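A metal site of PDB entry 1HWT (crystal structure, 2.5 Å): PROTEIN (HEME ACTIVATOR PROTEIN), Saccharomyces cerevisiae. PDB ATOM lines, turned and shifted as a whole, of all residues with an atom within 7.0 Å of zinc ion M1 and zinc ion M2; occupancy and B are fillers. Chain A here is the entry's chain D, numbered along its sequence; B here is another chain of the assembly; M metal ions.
The side-chain sulfur (SG) of Cys 20 sits close to the backbone NH (N) of Lys 22 (3.5 Å). The backbone NH of Cys 20 is in hydrogen-bond range of OP2 of DG 17 of chain B, 3.1 Å away. O of Cys 30 is in hydrogen-bond range of N of Ala 36 (3.3 Å). The backbone carbonyl oxygen (O) of Cys 30 is in hydrogen-bond range of the backbone NH (N) of Val 35 (2.8 Å). The side-chain sulfur (SG) of Cys 10 lies close to the backbone NH (N) of Ile 12 (3.8 Å). The side-chain sulfur (SG) of Cys 27 lies close to the backbone NH (N) of Gln 29 (3.7 Å). The backbone NH (N) of Val 18 is in hydrogen-bond range of the backbone carbonyl oxygen (O) of Cys 13 (2.9 Å). O of Cys 39 is in hydrogen-bond range of ND1 of His 26 (2.9 Å).
Within 4 Å of zinc ion M1: Cys 10, Cys 13, Cys 20 and Cys 27.
Within 4 Å of zinc ion M2: Cys 10, Cys 27, Cys 30 and Cys 39.
Zinc ion M1 is bound by the side-chain sulfur of Cys 20 (2.2 Å), the side-chain sulfur of Cys 13 (2.4 Å), the side-chain sulfur of Cys 10 (2.4 Å) and the side-chain sulfur of Cys 27 (2.4 Å). Zinc ion M1 has four donor atoms within binding distance.
Zinc ion M2 is bound by SG of Cys 30 (2.3 Å), SG of Cys 10 (2.3 Å), SG of Cys 27 (2.3 Å) and SG of Cys 39 (2.4 Å). Zinc ion M2 has four donor atoms within binding distance.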
ATOM      1  N   SER A   9      -7.901 -18.010   6.613  1.00  0.00           N
ATOM      2  CA  SER A   9      -8.794 -18.301   7.721  1.00  0.00           C
ATOM      3  C   SER A   9      -8.512 -17.276   8.804  1.00  0.00           C
ATOM      4  O   SER A   9      -7.472 -16.632   8.802  1.00  0.00           O
ATOM      5  CB  SER A   9      -8.538 -19.707   8.246  1.00  0.00           C
ATOM      6  OG  SER A   9      -8.220 -20.582   7.174  1.00  0.00           O
ATOM      7  N   CYS A  10      -9.452 -17.098   9.723  1.00  0.00           N
ATOM      8  CA  CYS A  10      -9.244 -16.128  10.787  1.00  0.00           C
ATOM      9  C   CYS A  10      -8.284 -16.692  11.821  1.00  0.00           C
ATOM     10  O   CYS A  10      -8.204 -17.898  12.033  1.00  0.00           O
ATOM     11  CB  CYS A  10     -10.564 -15.759  11.433  1.00  0.00           C
ATOM     12  SG  CYS A  10     -11.227 -17.037  12.519  1.00  0.00           S
ATOM     13  N   THR A  11      -7.540 -15.808  12.475  1.00  0.00           N
ATOM     14  CA  THR A  11      -6.575 -16.191  13.478  1.00  0.00           C
ATOM     15  C   THR A  11      -7.086 -17.167  14.535  1.00  0.00           C
ATOM     16  O   THR A  11      -6.363 -18.064  14.940  1.00  0.00           O
ATOM     17  CB  THR A  11      -6.007 -14.934  14.189  1.00  0.00           C
ATOM     18  OG1 THR A  11      -7.048 -14.291  14.941  1.00  0.00           O
ATOM     19  CG2 THR A  11      -5.441 -13.969  13.168  1.00  0.00           C
ATOM     20  N   ILE A  12      -8.335 -17.017  14.976  1.00  0.00           N
ATOM     21  CA  ILE A  12      -8.844 -17.908  15.997  1.00  0.00           C
ATOM     22  C   ILE A  12      -9.057 -19.314  15.489  1.00  0.00           C
ATOM     23  O   ILE A  12      -8.658 -20.278  16.135  1.00  0.00           O
ATOM     24  CB  ILE A  12     -10.161 -17.408  16.594  1.00  0.00           C
ATOM     25  CG1 ILE A  12      -9.987 -15.969  17.096  1.00  0.00           C
ATOM     26  CG2 ILE A  12     -10.611 -18.336  17.711  1.00  0.00           C
ATOM     27  CD1 ILE A  12     -10.032 -15.817  18.599  1.00  0.00           C
ATOM     28  N   CYS A  13      -9.698 -19.453  14.341  1.00  0.00           N
ATOM     29  CA  CYS A  13      -9.931 -20.778  13.779  1.00  0.00           C
ATOM     30  C   CYS A  13      -8.580 -21.441  13.540  1.00  0.00           C
ATOM     31  O   CYS A  13      -8.435 -22.631  13.780  1.00  0.00           O
ATOM     32  CB  CYS A  13     -10.693 -20.686  12.469  1.00  0.00           C
ATOM     33  SG  CYS A  13     -12.478 -20.489  12.697  1.00  0.00           S
ATOM     34  N   ARG A  14      -7.606 -20.671  13.080  1.00  0.00           N
ATOM     35  CA  ARG A  14      -6.274 -21.198  12.818  1.00  0.00           C
ATOM     36  C   ARG A  14      -5.586 -21.647  14.107  1.00  0.00           C
ATOM     37  O   ARG A  14      -4.957 -22.707  14.153  1.00  0.00           O
ATOM     38  CB  ARG A  14      -5.417 -20.130  12.130  1.00  0.00           C
ATOM     39  CG  ARG A  14      -4.541 -20.678  11.042  1.00  0.00           C
ATOM     40  CD  ARG A  14      -3.247 -19.933  10.936  1.00  0.00           C
ATOM     41  NE  ARG A  14      -3.376 -18.518  11.273  1.00  0.00           N
ATOM     42  CZ  ARG A  14      -2.742 -17.933  12.281  1.00  0.00           C
ATOM     43  NH1 ARG A  14      -1.935 -18.656  13.053  1.00  0.00           N
ATOM     44  NH2 ARG A  14      -2.892 -16.641  12.527  1.00  0.00           N
ATOM     45  N   VAL A  18      -9.850 -25.170  13.789  1.00  0.00           N
ATOM     46  CA  VAL A  18     -11.194 -25.591  13.495  1.00  0.00           C
ATOM     47  C   VAL A  18     -11.578 -25.114  12.105  1.00  0.00           C
ATOM     48  O   VAL A  18     -10.797 -24.452  11.433  1.00  0.00           O
ATOM     49  CB  VAL A  18     -12.156 -25.026  14.537  1.00  0.00           C
ATOM     50  CG1 VAL A  18     -11.867 -25.673  15.884  1.00  0.00           C
ATOM     51  CG2 VAL A  18     -11.991 -23.545  14.637  1.00  0.00           C
ATOM     52  N   LYS A  19     -12.778 -25.466  11.657  1.00  0.00           N
ATOM     53  CA  LYS A  19     -13.223 -25.063  10.327  1.00  0.00           C
ATOM     54  C   LYS A  19     -13.640 -23.622  10.307  1.00  0.00           C
ATOM     55  O   LYS A  19     -14.467 -23.205  11.125  1.00  0.00           O
ATOM     56  CB  LYS A  19     -14.408 -25.903   9.861  1.00  0.00           C
ATOM     57  CG  LYS A  19     -14.361 -26.242   8.392  1.00  0.00           C
ATOM     58  CD  LYS A  19     -15.593 -25.765   7.655  1.00  0.00           C
ATOM     59  CE  LYS A  19     -15.584 -26.258   6.216  1.00  0.00           C
ATOM     60  NZ  LYS A  19     -14.859 -27.567   6.068  1.00  0.00           N
ATOM     61  N   CYS A  20     -13.094 -22.861   9.365  1.00  0.00           N
ATOM     62  CA  CYS A  20     -13.423 -21.458   9.219  1.00  0.00           C
ATOM     63  C   CYS A  20     -14.275 -21.206   7.981  1.00  0.00           C
ATOM     64  O   CYS A  20     -13.911 -21.586   6.873  1.00  0.00           O
ATOM     65  CB  CYS A  20     -12.151 -20.618   9.139  1.00  0.00           C
ATOM     66  SG  CYS A  20     -12.449 -18.838   9.318  1.00  0.00           S
ATOM     67  N   ASP A  21     -15.407 -20.546   8.187  1.00  0.00           N
ATOM     68  CA  ASP A  21     -16.303 -20.223   7.090  1.00  0.00           C
ATOM     69  C   ASP A  21     -15.811 -18.973   6.354  1.00  0.00           C
ATOM     70  O   ASP A  21     -16.156 -18.749   5.199  1.00  0.00           O
ATOM     71  CB  ASP A  21     -17.706 -19.993   7.634  1.00  0.00           C
ATOM     72  CG  ASP A  21     -17.706 -19.171   8.884  1.00  0.00           C
ATOM     73  OD1 ASP A  21     -17.498 -19.737   9.978  1.00  0.00           O
ATOM     74  OD2 ASP A  21     -17.916 -17.945   8.773  1.00  0.00           O
ATOM     75  N   LYS A  22     -15.007 -18.163   7.043  1.00  0.00           N
ATOM     76  CA  LYS A  22     -14.421 -16.939   6.484  1.00  0.00           C
ATOM     77  C   LYS A  22     -15.306 -15.729   6.422  1.00  0.00           C
ATOM     78  O   LYS A  22     -14.920 -14.715   5.857  1.00  0.00           O
ATOM     79  CB  LYS A  22     -13.840 -17.212   5.108  1.00  0.00           C
ATOM     80  CG  LYS A  22     -12.745 -18.235   5.124  1.00  0.00           C
ATOM     81  CD  LYS A  22     -11.652 -17.874   4.184  1.00  0.00           C
ATOM     82  CE  LYS A  22     -11.339 -19.020   3.246  1.00  0.00           C
ATOM     83  NZ  LYS A  22     -11.560 -20.360   3.848  1.00  0.00           N
ATOM     84  N   LEU A  23     -16.497 -15.818   7.000  1.00  0.00           N
ATOM     85  CA  LEU A  23     -17.444 -14.706   7.018  1.00  0.00           C
ATOM     86  C   LEU A  23     -16.814 -13.395   7.497  1.00  0.00           C
ATOM     87  O   LEU A  23     -15.994 -13.406   8.414  1.00  0.00           O
ATOM     88  CB  LEU A  23     -18.620 -15.042   7.917  1.00  0.00           C
ATOM     89  CG  LEU A  23     -20.029 -14.997   7.331  1.00  0.00           C
ATOM     90  CD1 LEU A  23     -20.416 -13.553   7.041  1.00  0.00           C
ATOM     91  CD2 LEU A  23     -20.072 -15.883   6.094  1.00  0.00           C
ATOM     92  N   PRO A  25     -17.413  -9.313   8.979  1.00  0.00           N
ATOM     93  CA  PRO A  25     -16.053  -9.123   9.509  1.00  0.00           C
ATOM     94  C   PRO A  25     -15.622 -10.166  10.537  1.00  0.00           C
ATOM     95  O   PRO A  25     -14.439 -10.291  10.832  1.00  0.00           O
ATOM     96  CB  PRO A  25     -16.094  -7.721  10.085  1.00  0.00           C
ATOM     97  CG  PRO A  25     -17.519  -7.571  10.550  1.00  0.00           C
ATOM     98  CD  PRO A  25     -18.379  -8.452   9.672  1.00  0.00           C
ATOM     99  N   HIS A  26     -16.591 -10.884  11.092  1.00  0.00           N
ATOM    100  CA  HIS A  26     -16.337 -11.929  12.092  1.00  0.00           C
ATOM    101  C   HIS A  26     -16.996 -13.215  11.573  1.00  0.00           C
ATOM    102  O   HIS A  26     -18.140 -13.184  11.139  1.00  0.00           O
ATOM    103  CB  HIS A  26     -16.975 -11.550  13.419  1.00  0.00           C
ATOM    104  CG  HIS A  26     -16.536 -10.233  13.964  1.00  0.00           C
ATOM    105  ND1 HIS A  26     -15.250  -9.749  13.878  1.00  0.00           N
ATOM    106  CD2 HIS A  26     -17.210  -9.334  14.730  1.00  0.00           C
ATOM    107  CE1 HIS A  26     -15.197  -8.604  14.574  1.00  0.00           C
ATOM    108  NE2 HIS A  26     -16.364  -8.315  15.116  1.00  0.00           N
ATOM    109  N   CYS A  27     -16.291 -14.336  11.643  1.00  0.00           N
ATOM    110  CA  CYS A  27     -16.824 -15.601  11.121  1.00  0.00           C
ATOM    111  C   CYS A  27     -17.829 -16.293  12.002  1.00  0.00           C
ATOM    112  O   CYS A  27     -17.866 -16.075  13.213  1.00  0.00           O
ATOM    113  CB  CYS A  27     -15.669 -16.559  10.767  1.00  0.00           C
ATOM    114  SG  CYS A  27     -14.819 -17.400  12.161  1.00  0.00           S
ATOM    115  N   GLN A  28     -18.667 -17.124  11.372  1.00  0.00           N
ATOM    116  CA  GLN A  28     -19.732 -17.866  12.054  1.00  0.00           C
ATOM    117  C   GLN A  28     -19.186 -18.847  13.083  1.00  0.00           C
ATOM    118  O   GLN A  28     -19.865 -19.212  14.032  1.00  0.00           O
ATOM    119  CB  GLN A  28     -20.595 -18.626  11.045  1.00  0.00           C
ATOM    120  CG  GLN A  28     -21.778 -17.824  10.439  1.00  0.00           C
ATOM    121  CD  GLN A  28     -22.483 -16.905  11.456  1.00  0.00           C
ATOM    122  OE1 GLN A  28     -23.145 -17.374  12.400  1.00  0.00           O
ATOM    123  NE2 GLN A  28     -22.344 -15.581  11.261  1.00  0.00           N
ATOM    124  N   GLN A  29     -17.948 -19.302  12.874  1.00  0.00           N
ATOM    125  CA  GLN A  29     -17.348 -20.224  13.832  1.00  0.00           C
ATOM    126  C   GLN A  29     -17.106 -19.489  15.145  1.00  0.00           C
ATOM    127  O   GLN A  29     -17.448 -19.969  16.218  1.00  0.00           O
ATOM    128  CB  GLN A  29     -16.028 -20.764  13.276  1.00  0.00           C
ATOM    129  CG  GLN A  29     -15.323 -21.735  14.195  1.00  0.00           C
ATOM    130  CD  GLN A  29     -16.056 -23.061  14.298  1.00  0.00           C
ATOM    131  OE1 GLN A  29     -16.673 -23.355  15.313  1.00  0.00           O
ATOM    132  NE2 GLN A  29     -15.982 -23.857  13.237  1.00  0.00           N
ATOM    133  N   CYS A  30     -16.535 -18.297  15.049  1.00  0.00           N
ATOM    134  CA  CYS A  30     -16.262 -17.497  16.238  1.00  0.00           C
ATOM    135  C   CYS A  30     -17.545 -17.044  16.884  1.00  0.00           C
ATOM    136  O   CYS A  30     -17.665 -17.049  18.107  1.00  0.00           O
ATOM    137  CB  CYS A  30     -15.406 -16.289  15.871  1.00  0.00           C
ATOM    138  SG  CYS A  30     -13.650 -16.694  15.573  1.00  0.00           S
ATOM    139  N   THR A  31     -18.517 -16.650  16.071  1.00  0.00           N
ATOM    140  CA  THR A  31     -19.801 -16.193  16.590  1.00  0.00           C
ATOM    141  C   THR A  31     -20.521 -17.350  17.301  1.00  0.00           C
ATOM    142  O   THR A  31     -21.015 -17.192  18.413  1.00  0.00           O
ATOM    143  CB  THR A  31     -20.682 -15.679  15.459  1.00  0.00           C
ATOM    144  OG1 THR A  31     -20.037 -14.574  14.844  1.00  0.00           O
ATOM    145  CG2 THR A  31     -22.005 -15.233  15.985  1.00  0.00           C
ATOM    146  N   VAL A  35     -16.903 -15.884  20.578  1.00  0.00           N
ATOM    147  CA  VAL A  35     -15.737 -14.998  20.561  1.00  0.00           C
ATOM    148  C   VAL A  35     -15.732 -14.164  19.268  1.00  0.00           C
ATOM    149  O   VAL A  35     -14.679 -13.780  18.764  1.00  0.00           O
ATOM    150  CB  VAL A  35     -14.427 -15.814  20.655  1.00  0.00           C
ATOM    151  CG1 VAL A  35     -14.332 -16.457  22.014  1.00  0.00           C
ATOM    152  CG2 VAL A  35     -14.388 -16.876  19.580  1.00  0.00           C
ATOM    153  N   ALA A  36     -16.938 -13.893  18.758  1.00  0.00           N
ATOM    154  CA  ALA A  36     -17.135 -13.142  17.522  1.00  0.00           C
ATOM    155  C   ALA A  36     -16.200 -11.963  17.307  1.00  0.00           C
ATOM    156  O   ALA A  36     -15.494 -11.911  16.311  1.00  0.00           O
ATOM    157  CB  ALA A  36     -18.568 -12.663  17.429  1.00  0.00           C
ATOM    158  N   LEU A  38     -13.511 -11.259  18.518  1.00  0.00           N
ATOM    159  CA  LEU A  38     -12.096 -11.584  18.720  1.00  0.00           C
ATOM    160  C   LEU A  38     -11.610 -11.993  17.349  1.00  0.00           C
ATOM    161  O   LEU A  38     -10.411 -12.168  17.106  1.00  0.00           O
ATOM    162  CB  LEU A  38     -11.955 -12.760  19.687  1.00  0.00           C
ATOM    163  CG  LEU A  38     -11.302 -12.549  21.056  1.00  0.00           C
ATOM    164  CD1 LEU A  38     -11.852 -11.320  21.730  1.00  0.00           C
ATOM    165  CD2 LEU A  38     -11.578 -13.758  21.912  1.00  0.00           C
ATOM    166  N   CYS A  39     -12.571 -12.126  16.440  1.00  0.00           N
ATOM    167  CA  CYS A  39     -12.311 -12.562  15.074  1.00  0.00           C
ATOM    168  C   CYS A  39     -11.789 -11.511  14.110  1.00  0.00           C
ATOM    169  O   CYS A  39     -12.388 -10.454  13.945  1.00  0.00           O
ATOM    170  CB  CYS A  39     -13.577 -13.148  14.482  1.00  0.00           C
ATOM    171  SG  CYS A  39     -13.283 -13.952  12.892  1.00  0.00           S
ATOM    172  N   HIS A  40     -10.669 -11.825  13.461  1.00  0.00           N
ATOM    173  CA  HIS A  40     -10.069 -10.949  12.478  1.00  0.00           C
ATOM    174  C   HIS A  40      -9.163 -11.749  11.567  1.00  0.00           C
ATOM    175  O   HIS A  40      -8.822 -12.875  11.867  1.00  0.00           O
ATOM    176  CB  HIS A  40      -9.306  -9.812  13.157  1.00  0.00           C
ATOM    177  CG  HIS A  40      -8.160 -10.256  14.006  1.00  0.00           C
ATOM    178  ND1 HIS A  40      -8.315 -10.633  15.323  1.00  0.00           N
ATOM    179  CD2 HIS A  40      -6.837 -10.335  13.742  1.00  0.00           C
ATOM    180  CE1 HIS A  40      -7.135 -10.919  15.836  1.00  0.00           C
ATOM    181  NE2 HIS A  40      -6.218 -10.748  14.902  1.00  0.00           N
ATOM    182  N   TYR A  41      -8.796 -11.152  10.432  1.00  0.00           N
ATOM    183  CA  TYR A  41      -7.967 -11.833   9.449  1.00  0.00           C
ATOM    184  C   TYR A  41      -6.654 -11.125   9.167  1.00  0.00           C
ATOM    185  O   TYR A  41      -6.551  -9.909   9.310  1.00  0.00           O
ATOM    186  CB  TYR A  41      -8.743 -11.974   8.137  1.00  0.00           C
ATOM    187  CG  TYR A  41     -10.077 -12.666   8.268  1.00  0.00           C
ATOM    188  CD1 TYR A  41     -11.187 -11.992   8.800  1.00  0.00           C
ATOM    189  CD2 TYR A  41     -10.222 -13.991   7.884  1.00  0.00           C
ATOM    190  CE1 TYR A  41     -12.401 -12.637   8.930  1.00  0.00           C
ATOM    191  CE2 TYR A  41     -11.442 -14.638   8.022  1.00  0.00           C
ATOM    192  CZ  TYR A  41     -12.524 -13.954   8.540  1.00  0.00           C
ATOM    193  OH  TYR A  41     -13.729 -14.608   8.636  1.00  0.00           O
ATOM    194  P    DG B  17     -10.733 -24.842   6.788  1.00  0.00           P
ATOM    195  OP1  DG B  17     -11.917 -25.038   5.900  1.00  0.00           O
ATOM    196  OP2  DG B  17     -10.680 -23.663   7.672  1.00  0.00           O
ATOM    197  O5'  DG B  17     -10.575 -26.143   7.641  1.00  0.00           O
ATOM    198  C5'  DG B  17     -10.571 -27.395   6.993  1.00  0.00           C
ATOM    199  C4'  DG B  17     -10.405 -28.494   8.001  1.00  0.00           C
ATOM    200  O4'  DG B  17      -9.024 -28.615   8.367  1.00  0.00           O
ATOM    201  C3'  DG B  17     -11.190 -28.338   9.307  1.00  0.00           C
ATOM    202  O3'  DG B  17     -11.648 -29.646   9.566  1.00  0.00           O
ATOM    203  C2'  DG B  17     -10.111 -27.975  10.308  1.00  0.00           C
ATOM    204  C1'  DG B  17      -8.947 -28.780   9.764  1.00  0.00           C
ATOM    205  N9   DG B  17      -7.586 -28.415  10.155  1.00  0.00           N
ATOM    206  C8   DG B  17      -7.130 -27.224  10.689  1.00  0.00           C
ATOM    207  N7   DG B  17      -5.845 -27.235  10.927  1.00  0.00           N
ATOM    208  C5   DG B  17      -5.437 -28.500  10.534  1.00  0.00           C
ATOM    209  C6   DG B  17      -4.150 -29.085  10.539  1.00  0.00           C
ATOM    210  O6   DG B  17      -3.086 -28.592  10.879  1.00  0.00           O
ATOM    211  N1   DG B  17      -4.180 -30.376  10.059  1.00  0.00           N
ATOM    212  C2   DG B  17      -5.303 -31.031   9.616  1.00  0.00           C
ATOM    213  N2   DG B  17      -5.131 -32.288   9.218  1.00  0.00           N
ATOM    214  N3   DG B  17      -6.500 -30.485   9.588  1.00  0.00           N
ATOM    215  C4   DG B  17      -6.495 -29.230  10.064  1.00  0.00           C
HETATM  216 ZN    ZN M   1     -12.810 -18.490  11.502  1.00  0.00          ZN
HETATM  217 ZN    ZN M   2     -13.213 -16.249  13.399  1.00  0.00          ZN
